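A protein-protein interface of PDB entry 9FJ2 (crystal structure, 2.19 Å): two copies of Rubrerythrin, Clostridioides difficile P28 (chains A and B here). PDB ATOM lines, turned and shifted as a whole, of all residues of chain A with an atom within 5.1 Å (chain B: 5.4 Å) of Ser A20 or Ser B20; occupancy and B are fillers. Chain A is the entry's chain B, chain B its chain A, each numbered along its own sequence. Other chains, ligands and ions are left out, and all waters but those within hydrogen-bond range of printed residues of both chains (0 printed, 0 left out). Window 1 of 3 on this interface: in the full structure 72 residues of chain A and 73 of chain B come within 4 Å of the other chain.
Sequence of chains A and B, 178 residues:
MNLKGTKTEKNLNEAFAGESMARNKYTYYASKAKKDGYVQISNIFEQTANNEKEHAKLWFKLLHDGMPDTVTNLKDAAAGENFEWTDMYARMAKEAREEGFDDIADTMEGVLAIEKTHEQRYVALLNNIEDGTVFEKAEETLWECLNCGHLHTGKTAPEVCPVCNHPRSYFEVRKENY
Printed residues of chain B within 4 Å of Ala A17: Met B21 (3.6 Å). Gly A18 touches none of the printed residues of chain B. Ser A20 touches just these residues of chain B: Ser B20 (3.4 Å), Met B21 (3.7 Å) and Asn B24 (2.8 Å). Of the printed residues of chain B, Ala A56 touches Asn B24 (3.7 Å). Ala B15 touches none of the printed residues of chain A. Of the printed residues of chain A, Phe B16 touches Met A21 (3.9 Å) and Asn A24 (3.998 Å). Of the printed residues of chain A, Ser B20 touches Ser A20 (3.4 Å), Met A21 (3.9 Å) and Asn A24 (2.8 Å). Printed residues of chain A within 4 Å of Arg B23: Arg A23 and Asn A24. The nearest printed residue of chain A that does not touch Ser B20 is Ala A17 (5.3 Å).
Among the printed residues, merely in contact across the chains: Phe A16 with Met B21 (3.6 Å), Phe A16 with Asn B24 (3.96 Å), Phe A16 with Lys B25 (3.9 Å), Ala A17 with Met B21 (3.6 Å), Ser A20 with Ser B20 (3.4 Å), Ser A20 with Met B21 (3.7 Å), Met A21 with Phe B16 (3.9 Å), Met A21 with Ala B17 (3.7 Å), Met A21 with Ser B20 (3.9 Å), Asn A24 with Phe B16 (3.998 Å), Asn A24 with Ala B56 (3.4 Å) and Ala A56 with Asn B24 (3.7 Å).
Of the 11 printed residues of chain A, 7 touch a printed residue of chain B. Printed residues of chain A that touch a printed residue of chain B: Phe A16, Ala A17, Ser A20, Met A21, Arg A23, Asn A24 and Ala A56. Hydrophobic or aromatic side chains of chain A within 4 Å of the printed part of chain B: Phe A16, Ala A17, Met A21 and Ala A56.
Phe A16 touches Met B21, and with the chains exchanged Met A21 touches Phe B16. Ser A20 touches Met B21, and with the chains exchanged Met A21 touches Ser B20. Arg A23 touches its own counterpart, Arg B23. Asn A24 touches Ala B56, and with the chains exchanged Ala A56 touches Asn B24. 11 positions are printed for both chains. Of the 17 pairs that touch across the chains among the printed residues, 16 have their exchanged pair printed and touching as well.
OG of Ser A20 lies within hydrogen-bond range of O of Phe A16, 2.9 Å away. The backbone carbonyl oxygen (O) of Phe B16 sits at hydrogen-bond distance from the side-chain hydroxyl (OG) of Ser B20 (2.7 Å).
OD1 of Asn A24 lies within hydrogen-bond range of NH1 of Arg B23 (2.8 Å). The side-chain hydroxyl (OG) of Ser A20 is in hydrogen-bond range of the side-chain amide nitrogen (ND2) of Asn B24 (2.8 Å). The side-chain hydroxyl (OG) of Ser B20 is in hydrogen-bond range of the side-chain amide nitrogen (ND2) of Asn A24 (2.8 Å). NH1 of Arg A23 sits at hydrogen-bond distance from OD1 of Asn B24 (3.3 Å). NH2 of Arg B23 sits close to NH2 of Arg A23, at 3.4 Å.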
ATOM      1  N   ALA A  15      23.154  33.031  34.661  1.00  0.00           N
ATOM      2  CA  ALA A  15      24.090  31.960  34.344  1.00  0.00           C
ATOM      3  C   ALA A  15      23.531  31.029  33.276  1.00  0.00           C
ATOM      4  O   ALA A  15      24.290  30.509  32.448  1.00  0.00           O
ATOM      5  CB  ALA A  15      24.442  31.171  35.611  1.00  0.00           C
ATOM      6  N   PHE A  16      22.213  30.813  33.269  1.00  0.00           N
ATOM      7  CA  PHE A  16      21.613  29.985  32.229  1.00  0.00           C
ATOM      8  C   PHE A  16      21.764  30.624  30.856  1.00  0.00           C
ATOM      9  O   PHE A  16      21.944  29.913  29.861  1.00  0.00           O
ATOM     10  CB  PHE A  16      20.137  29.725  32.537  1.00  0.00           C
ATOM     11  CG  PHE A  16      19.466  28.799  31.557  1.00  0.00           C
ATOM     12  CD1 PHE A  16      18.336  29.200  30.861  1.00  0.00           C
ATOM     13  CD2 PHE A  16      19.968  27.528  31.329  1.00  0.00           C
ATOM     14  CE1 PHE A  16      17.719  28.350  29.958  1.00  0.00           C
ATOM     15  CE2 PHE A  16      19.356  26.674  30.428  1.00  0.00           C
ATOM     16  CZ  PHE A  16      18.231  27.086  29.741  1.00  0.00           C
ATOM     17  N   ALA A  17      21.710  31.956  30.785  1.00  0.00           N
ATOM     18  CA  ALA A  17      21.870  32.642  29.507  1.00  0.00           C
ATOM     19  C   ALA A  17      23.302  32.535  28.999  1.00  0.00           C
ATOM     20  O   ALA A  17      23.533  32.225  27.824  1.00  0.00           O
ATOM     21  CB  ALA A  17      21.461  34.109  29.646  1.00  0.00           C
ATOM     22  N   GLY A  18      24.278  32.791  29.872  1.00  0.00           N
ATOM     23  CA  GLY A  18      25.666  32.780  29.441  1.00  0.00           C
ATOM     24  C   GLY A  18      26.143  31.404  29.015  1.00  0.00           C
ATOM     25  O   GLY A  18      26.844  31.266  28.009  1.00  0.00           O
ATOM     26  N   GLU A  19      25.775  30.369  29.774  1.00  0.00           N
ATOM     27  CA  GLU A  19      26.157  29.013  29.397  1.00  0.00           C
ATOM     28  C   GLU A  19      25.486  28.582  28.100  1.00  0.00           C
ATOM     29  O   GLU A  19      26.081  27.832  27.318  1.00  0.00           O
ATOM     30  CB  GLU A  19      25.819  28.037  30.524  1.00  0.00           C
ATOM     31  CG  GLU A  19      26.624  28.253  31.797  1.00  0.00           C
ATOM     32  CD  GLU A  19      28.003  27.615  31.740  1.00  0.00           C
ATOM     33  OE1 GLU A  19      28.268  26.875  30.769  1.00  0.00           O
ATOM     34  OE2 GLU A  19      28.801  27.865  32.666  1.00  0.00           O
ATOM     35  N   SER A  20      24.257  29.047  27.853  1.00  0.00           N
ATOM     36  CA  SER A  20      23.582  28.734  26.597  1.00  0.00           C
ATOM     37  C   SER A  20      24.266  29.415  25.418  1.00  0.00           C
ATOM     38  O   SER A  20      24.381  28.825  24.337  1.00  0.00           O
ATOM     39  CB  SER A  20      22.111  29.141  26.669  1.00  0.00           C
ATOM     40  OG  SER A  20      21.390  28.311  27.563  1.00  0.00           O
ATOM     41  N   MET A  21      24.718  30.659  25.603  1.00  0.00           N
ATOM     42  CA  MET A  21      25.434  31.347  24.534  1.00  0.00           C
ATOM     43  C   MET A  21      26.755  30.654  24.225  1.00  0.00           C
ATOM     44  O   MET A  21      27.135  30.525  23.055  1.00  0.00           O
ATOM     45  CB  MET A  21      25.671  32.810  24.913  1.00  0.00           C
ATOM     46  CG  MET A  21      24.403  33.649  25.004  1.00  0.00           C
ATOM     47  SD  MET A  21      24.731  35.407  25.256  1.00  0.00           S
ATOM     48  CE  MET A  21      24.124  35.620  26.926  1.00  0.00           C
ATOM     49  N   ALA A  22      27.466  30.199  25.260  1.00  0.00           N
ATOM     50  CA  ALA A  22      28.724  29.495  25.037  1.00  0.00           C
ATOM     51  C   ALA A  22      28.504  28.156  24.348  1.00  0.00           C
ATOM     52  O   ALA A  22      29.349  27.722  23.556  1.00  0.00           O
ATOM     53  CB  ALA A  22      29.461  29.298  26.363  1.00  0.00           C
ATOM     54  N   ARG A  23      27.381  27.488  24.632  1.00  0.00           N
ATOM     55  CA  ARG A  23      27.066  26.251  23.924  1.00  0.00           C
ATOM     56  C   ARG A  23      26.865  26.507  22.437  1.00  0.00           C
ATOM     57  O   ARG A  23      27.278  25.699  21.598  1.00  0.00           O
ATOM     58  CB  ARG A  23      25.823  25.597  24.527  1.00  0.00           C
ATOM     59  CG  ARG A  23      25.574  24.184  24.021  1.00  0.00           C
ATOM     60  CD  ARG A  23      24.095  23.837  24.026  1.00  0.00           C
ATOM     61  NE  ARG A  23      23.836  22.569  23.352  1.00  0.00           N
ATOM     62  CZ  ARG A  23      22.632  22.150  22.974  1.00  0.00           C
ATOM     63  NH1 ARG A  23      21.563  22.901  23.202  1.00  0.00           N
ATOM     64  NH2 ARG A  23      22.496  20.980  22.367  1.00  0.00           N
ATOM     65  N   ASN A  24      26.230  27.628  22.091  1.00  0.00           N
ATOM     66  CA  ASN A  24      26.084  27.983  20.685  1.00  0.00           C
ATOM     67  C   ASN A  24      27.406  28.461  20.101  1.00  0.00           C
ATOM     68  O   ASN A  24      27.720  28.171  18.940  1.00  0.00           O
ATOM     69  CB  ASN A  24      25.003  29.050  20.519  1.00  0.00           C
ATOM     70  CG  ASN A  24      23.676  28.469  20.076  1.00  0.00           C
ATOM     71  OD1 ASN A  24      23.606  27.323  19.630  1.00  0.00           O
ATOM     72  ND2 ASN A  24      22.613  29.256  20.198  1.00  0.00           N
ATOM     73  N   ALA A  56      24.427  24.570  32.037  1.00  0.00           N
ATOM     74  CA  ALA A  56      23.136  25.243  31.958  1.00  0.00           C
ATOM     75  C   ALA A  56      22.015  24.363  32.492  1.00  0.00           C
ATOM     76  O   ALA A  56      21.026  24.878  33.027  1.00  0.00           O
ATOM     77  CB  ALA A  56      22.850  25.660  30.515  1.00  0.00           C
ATOM     78  N   ALA B  15      19.050  39.076  21.219  1.00  0.00           N
ATOM     79  CA  ALA B  15      18.458  38.030  20.399  1.00  0.00           C
ATOM     80  C   ALA B  15      19.341  36.792  20.331  1.00  0.00           C
ATOM     81  O   ALA B  15      18.823  35.678  20.202  1.00  0.00           O
ATOM     82  CB  ALA B  15      18.181  38.561  18.991  1.00  0.00           C
ATOM     83  N   PHE B  16      20.665  36.958  20.406  1.00  0.00           N
ATOM     84  CA  PHE B  16      21.540  35.794  20.483  1.00  0.00           C
ATOM     85  C   PHE B  16      21.251  34.988  21.742  1.00  0.00           C
ATOM     86  O   PHE B  16      21.173  33.755  21.695  1.00  0.00           O
ATOM     87  CB  PHE B  16      23.006  36.224  20.438  1.00  0.00           C
ATOM     88  CG  PHE B  16      23.970  35.078  20.301  1.00  0.00           C
ATOM     89  CD1 PHE B  16      23.908  34.228  19.207  1.00  0.00           C
ATOM     90  CD2 PHE B  16      24.935  34.846  21.269  1.00  0.00           C
ATOM     91  CE1 PHE B  16      24.789  33.169  19.082  1.00  0.00           C
ATOM     92  CE2 PHE B  16      25.820  33.790  21.150  1.00  0.00           C
ATOM     93  CZ  PHE B  16      25.747  32.951  20.055  1.00  0.00           C
ATOM     94  N   ALA B  17      21.084  35.667  22.873  1.00  0.00           N
ATOM     95  CA  ALA B  17      20.525  35.026  24.051  1.00  0.00           C
ATOM     96  C   ALA B  17      19.028  34.805  23.855  1.00  0.00           C
ATOM     97  O   ALA B  17      18.398  35.387  22.967  1.00  0.00           O
ATOM     98  CB  ALA B  17      20.779  35.869  25.299  1.00  0.00           C
ATOM     99  N   GLY B  18      18.455  33.950  24.694  1.00  0.00           N
ATOM    100  CA  GLY B  18      17.063  33.582  24.527  1.00  0.00           C
ATOM    101  C   GLY B  18      16.904  32.570  23.414  1.00  0.00           C
ATOM    102  O   GLY B  18      16.411  31.461  23.637  1.00  0.00           O
ATOM    103  N   GLU B  19      17.316  32.953  22.203  1.00  0.00           N
ATOM    104  CA  GLU B  19      17.458  31.980  21.126  1.00  0.00           C
ATOM    105  C   GLU B  19      18.419  30.866  21.526  1.00  0.00           C
ATOM    106  O   GLU B  19      18.146  29.683  21.291  1.00  0.00           O
ATOM    107  CB  GLU B  19      17.939  32.680  19.855  1.00  0.00           C
ATOM    108  CG  GLU B  19      17.685  31.903  18.578  1.00  0.00           C
ATOM    109  CD  GLU B  19      16.219  31.876  18.198  1.00  0.00           C
ATOM    110  OE1 GLU B  19      15.706  32.896  17.690  1.00  0.00           O
ATOM    111  OE2 GLU B  19      15.578  30.828  18.410  1.00  0.00           O
ATOM    112  N   SER B  20      19.547  31.227  22.143  1.00  0.00           N
ATOM    113  CA  SER B  20      20.446  30.218  22.693  1.00  0.00           C
ATOM    114  C   SER B  20      19.835  29.538  23.910  1.00  0.00           C
ATOM    115  O   SER B  20      20.065  28.343  24.131  1.00  0.00           O
ATOM    116  CB  SER B  20      21.789  30.851  23.060  1.00  0.00           C
ATOM    117  OG  SER B  20      22.413  31.423  21.924  1.00  0.00           O
ATOM    118  N   MET B  21      19.056  30.277  24.704  1.00  0.00           N
ATOM    119  CA  MET B  21      18.391  29.680  25.858  1.00  0.00           C
ATOM    120  C   MET B  21      17.257  28.753  25.436  1.00  0.00           C
ATOM    121  O   MET B  21      16.984  27.760  26.122  1.00  0.00           O
ATOM    122  CB  MET B  21      17.869  30.776  26.789  1.00  0.00           C
ATOM    123  CG  MET B  21      18.857  31.189  27.873  1.00  0.00           C
ATOM    124  SD  MET B  21      18.220  32.462  28.984  1.00  0.00           S
ATOM    125  CE  MET B  21      18.263  33.906  27.929  1.00  0.00           C
ATOM    126  N   ALA B  22      16.589  29.053  24.319  1.00  0.00           N
ATOM    127  CA  ALA B  22      15.530  28.171  23.842  1.00  0.00           C
ATOM    128  C   ALA B  22      16.082  26.845  23.331  1.00  0.00           C
ATOM    129  O   ALA B  22      15.434  25.806  23.493  1.00  0.00           O
ATOM    130  CB  ALA B  22      14.713  28.863  22.751  1.00  0.00           C
ATOM    131  N   ARG B  23      17.264  26.855  22.709  1.00  0.00           N
ATOM    132  CA  ARG B  23      17.854  25.604  22.242  1.00  0.00           C
ATOM    133  C   ARG B  23      18.189  24.678  23.405  1.00  0.00           C
ATOM    134  O   ARG B  23      17.945  23.468  23.336  1.00  0.00           O
ATOM    135  CB  ARG B  23      19.098  25.886  21.398  1.00  0.00           C
ATOM    136  CG  ARG B  23      19.726  24.632  20.798  1.00  0.00           C
ATOM    137  CD  ARG B  23      21.115  24.905  20.232  1.00  0.00           C
ATOM    138  NE  ARG B  23      21.811  23.675  19.876  1.00  0.00           N
ATOM    139  CZ  ARG B  23      23.132  23.532  19.884  1.00  0.00           C
ATOM    140  NH1 ARG B  23      23.916  24.555  20.193  1.00  0.00           N
ATOM    141  NH2 ARG B  23      23.674  22.370  19.548  1.00  0.00           N
ATOM    142  N   ASN B  24      18.748  25.229  24.486  1.00  0.00           N
ATOM    143  CA  ASN B  24      19.011  24.408  25.664  1.00  0.00           C
ATOM    144  C   ASN B  24      17.713  23.935  26.303  1.00  0.00           C
ATOM    145  O   ASN B  24      17.616  22.782  26.740  1.00  0.00           O
ATOM    146  CB  ASN B  24      19.859  25.180  26.673  1.00  0.00           C
ATOM    147  CG  ASN B  24      21.321  24.783  26.627  1.00  0.00           C
ATOM    148  OD1 ASN B  24      21.649  23.617  26.415  1.00  0.00           O
ATOM    149  ND2 ASN B  24      22.206  25.748  26.844  1.00  0.00           N
ATOM    150  N   LYS B  25      16.702  24.807  26.356  1.00  0.00           N
ATOM    151  CA  LYS B  25      15.417  24.422  26.932  1.00  0.00           C
ATOM    152  C   LYS B  25      14.760  23.313  26.122  1.00  0.00           C
ATOM    153  O   LYS B  25      14.234  22.347  26.689  1.00  0.00           O
ATOM    154  CB  LYS B  25      14.494  25.639  27.017  1.00  0.00           C
ATOM    155  CG  LYS B  25      14.678  26.478  28.270  1.00  0.00           C
ATOM    156  CD  LYS B  25      13.439  27.309  28.562  1.00  0.00           C
ATOM    157  CE  LYS B  25      13.194  28.336  27.465  1.00  0.00           C
ATOM    158  NZ  LYS B  25      11.805  28.878  27.507  1.00  0.00           N
ATOM    159  N   ALA B  56      20.041  31.753  16.042  1.00  0.00           N
ATOM    160  CA  ALA B  56      21.090  32.419  16.803  1.00  0.00           C
ATOM    161  C   ALA B  56      22.367  32.550  15.988  1.00  0.00           C
ATOM    162  O   ALA B  56      23.127  33.506  16.180  1.00  0.00           O
ATOM    163  CB  ALA B  56      21.364  31.661  18.103  1.00  0.00           C
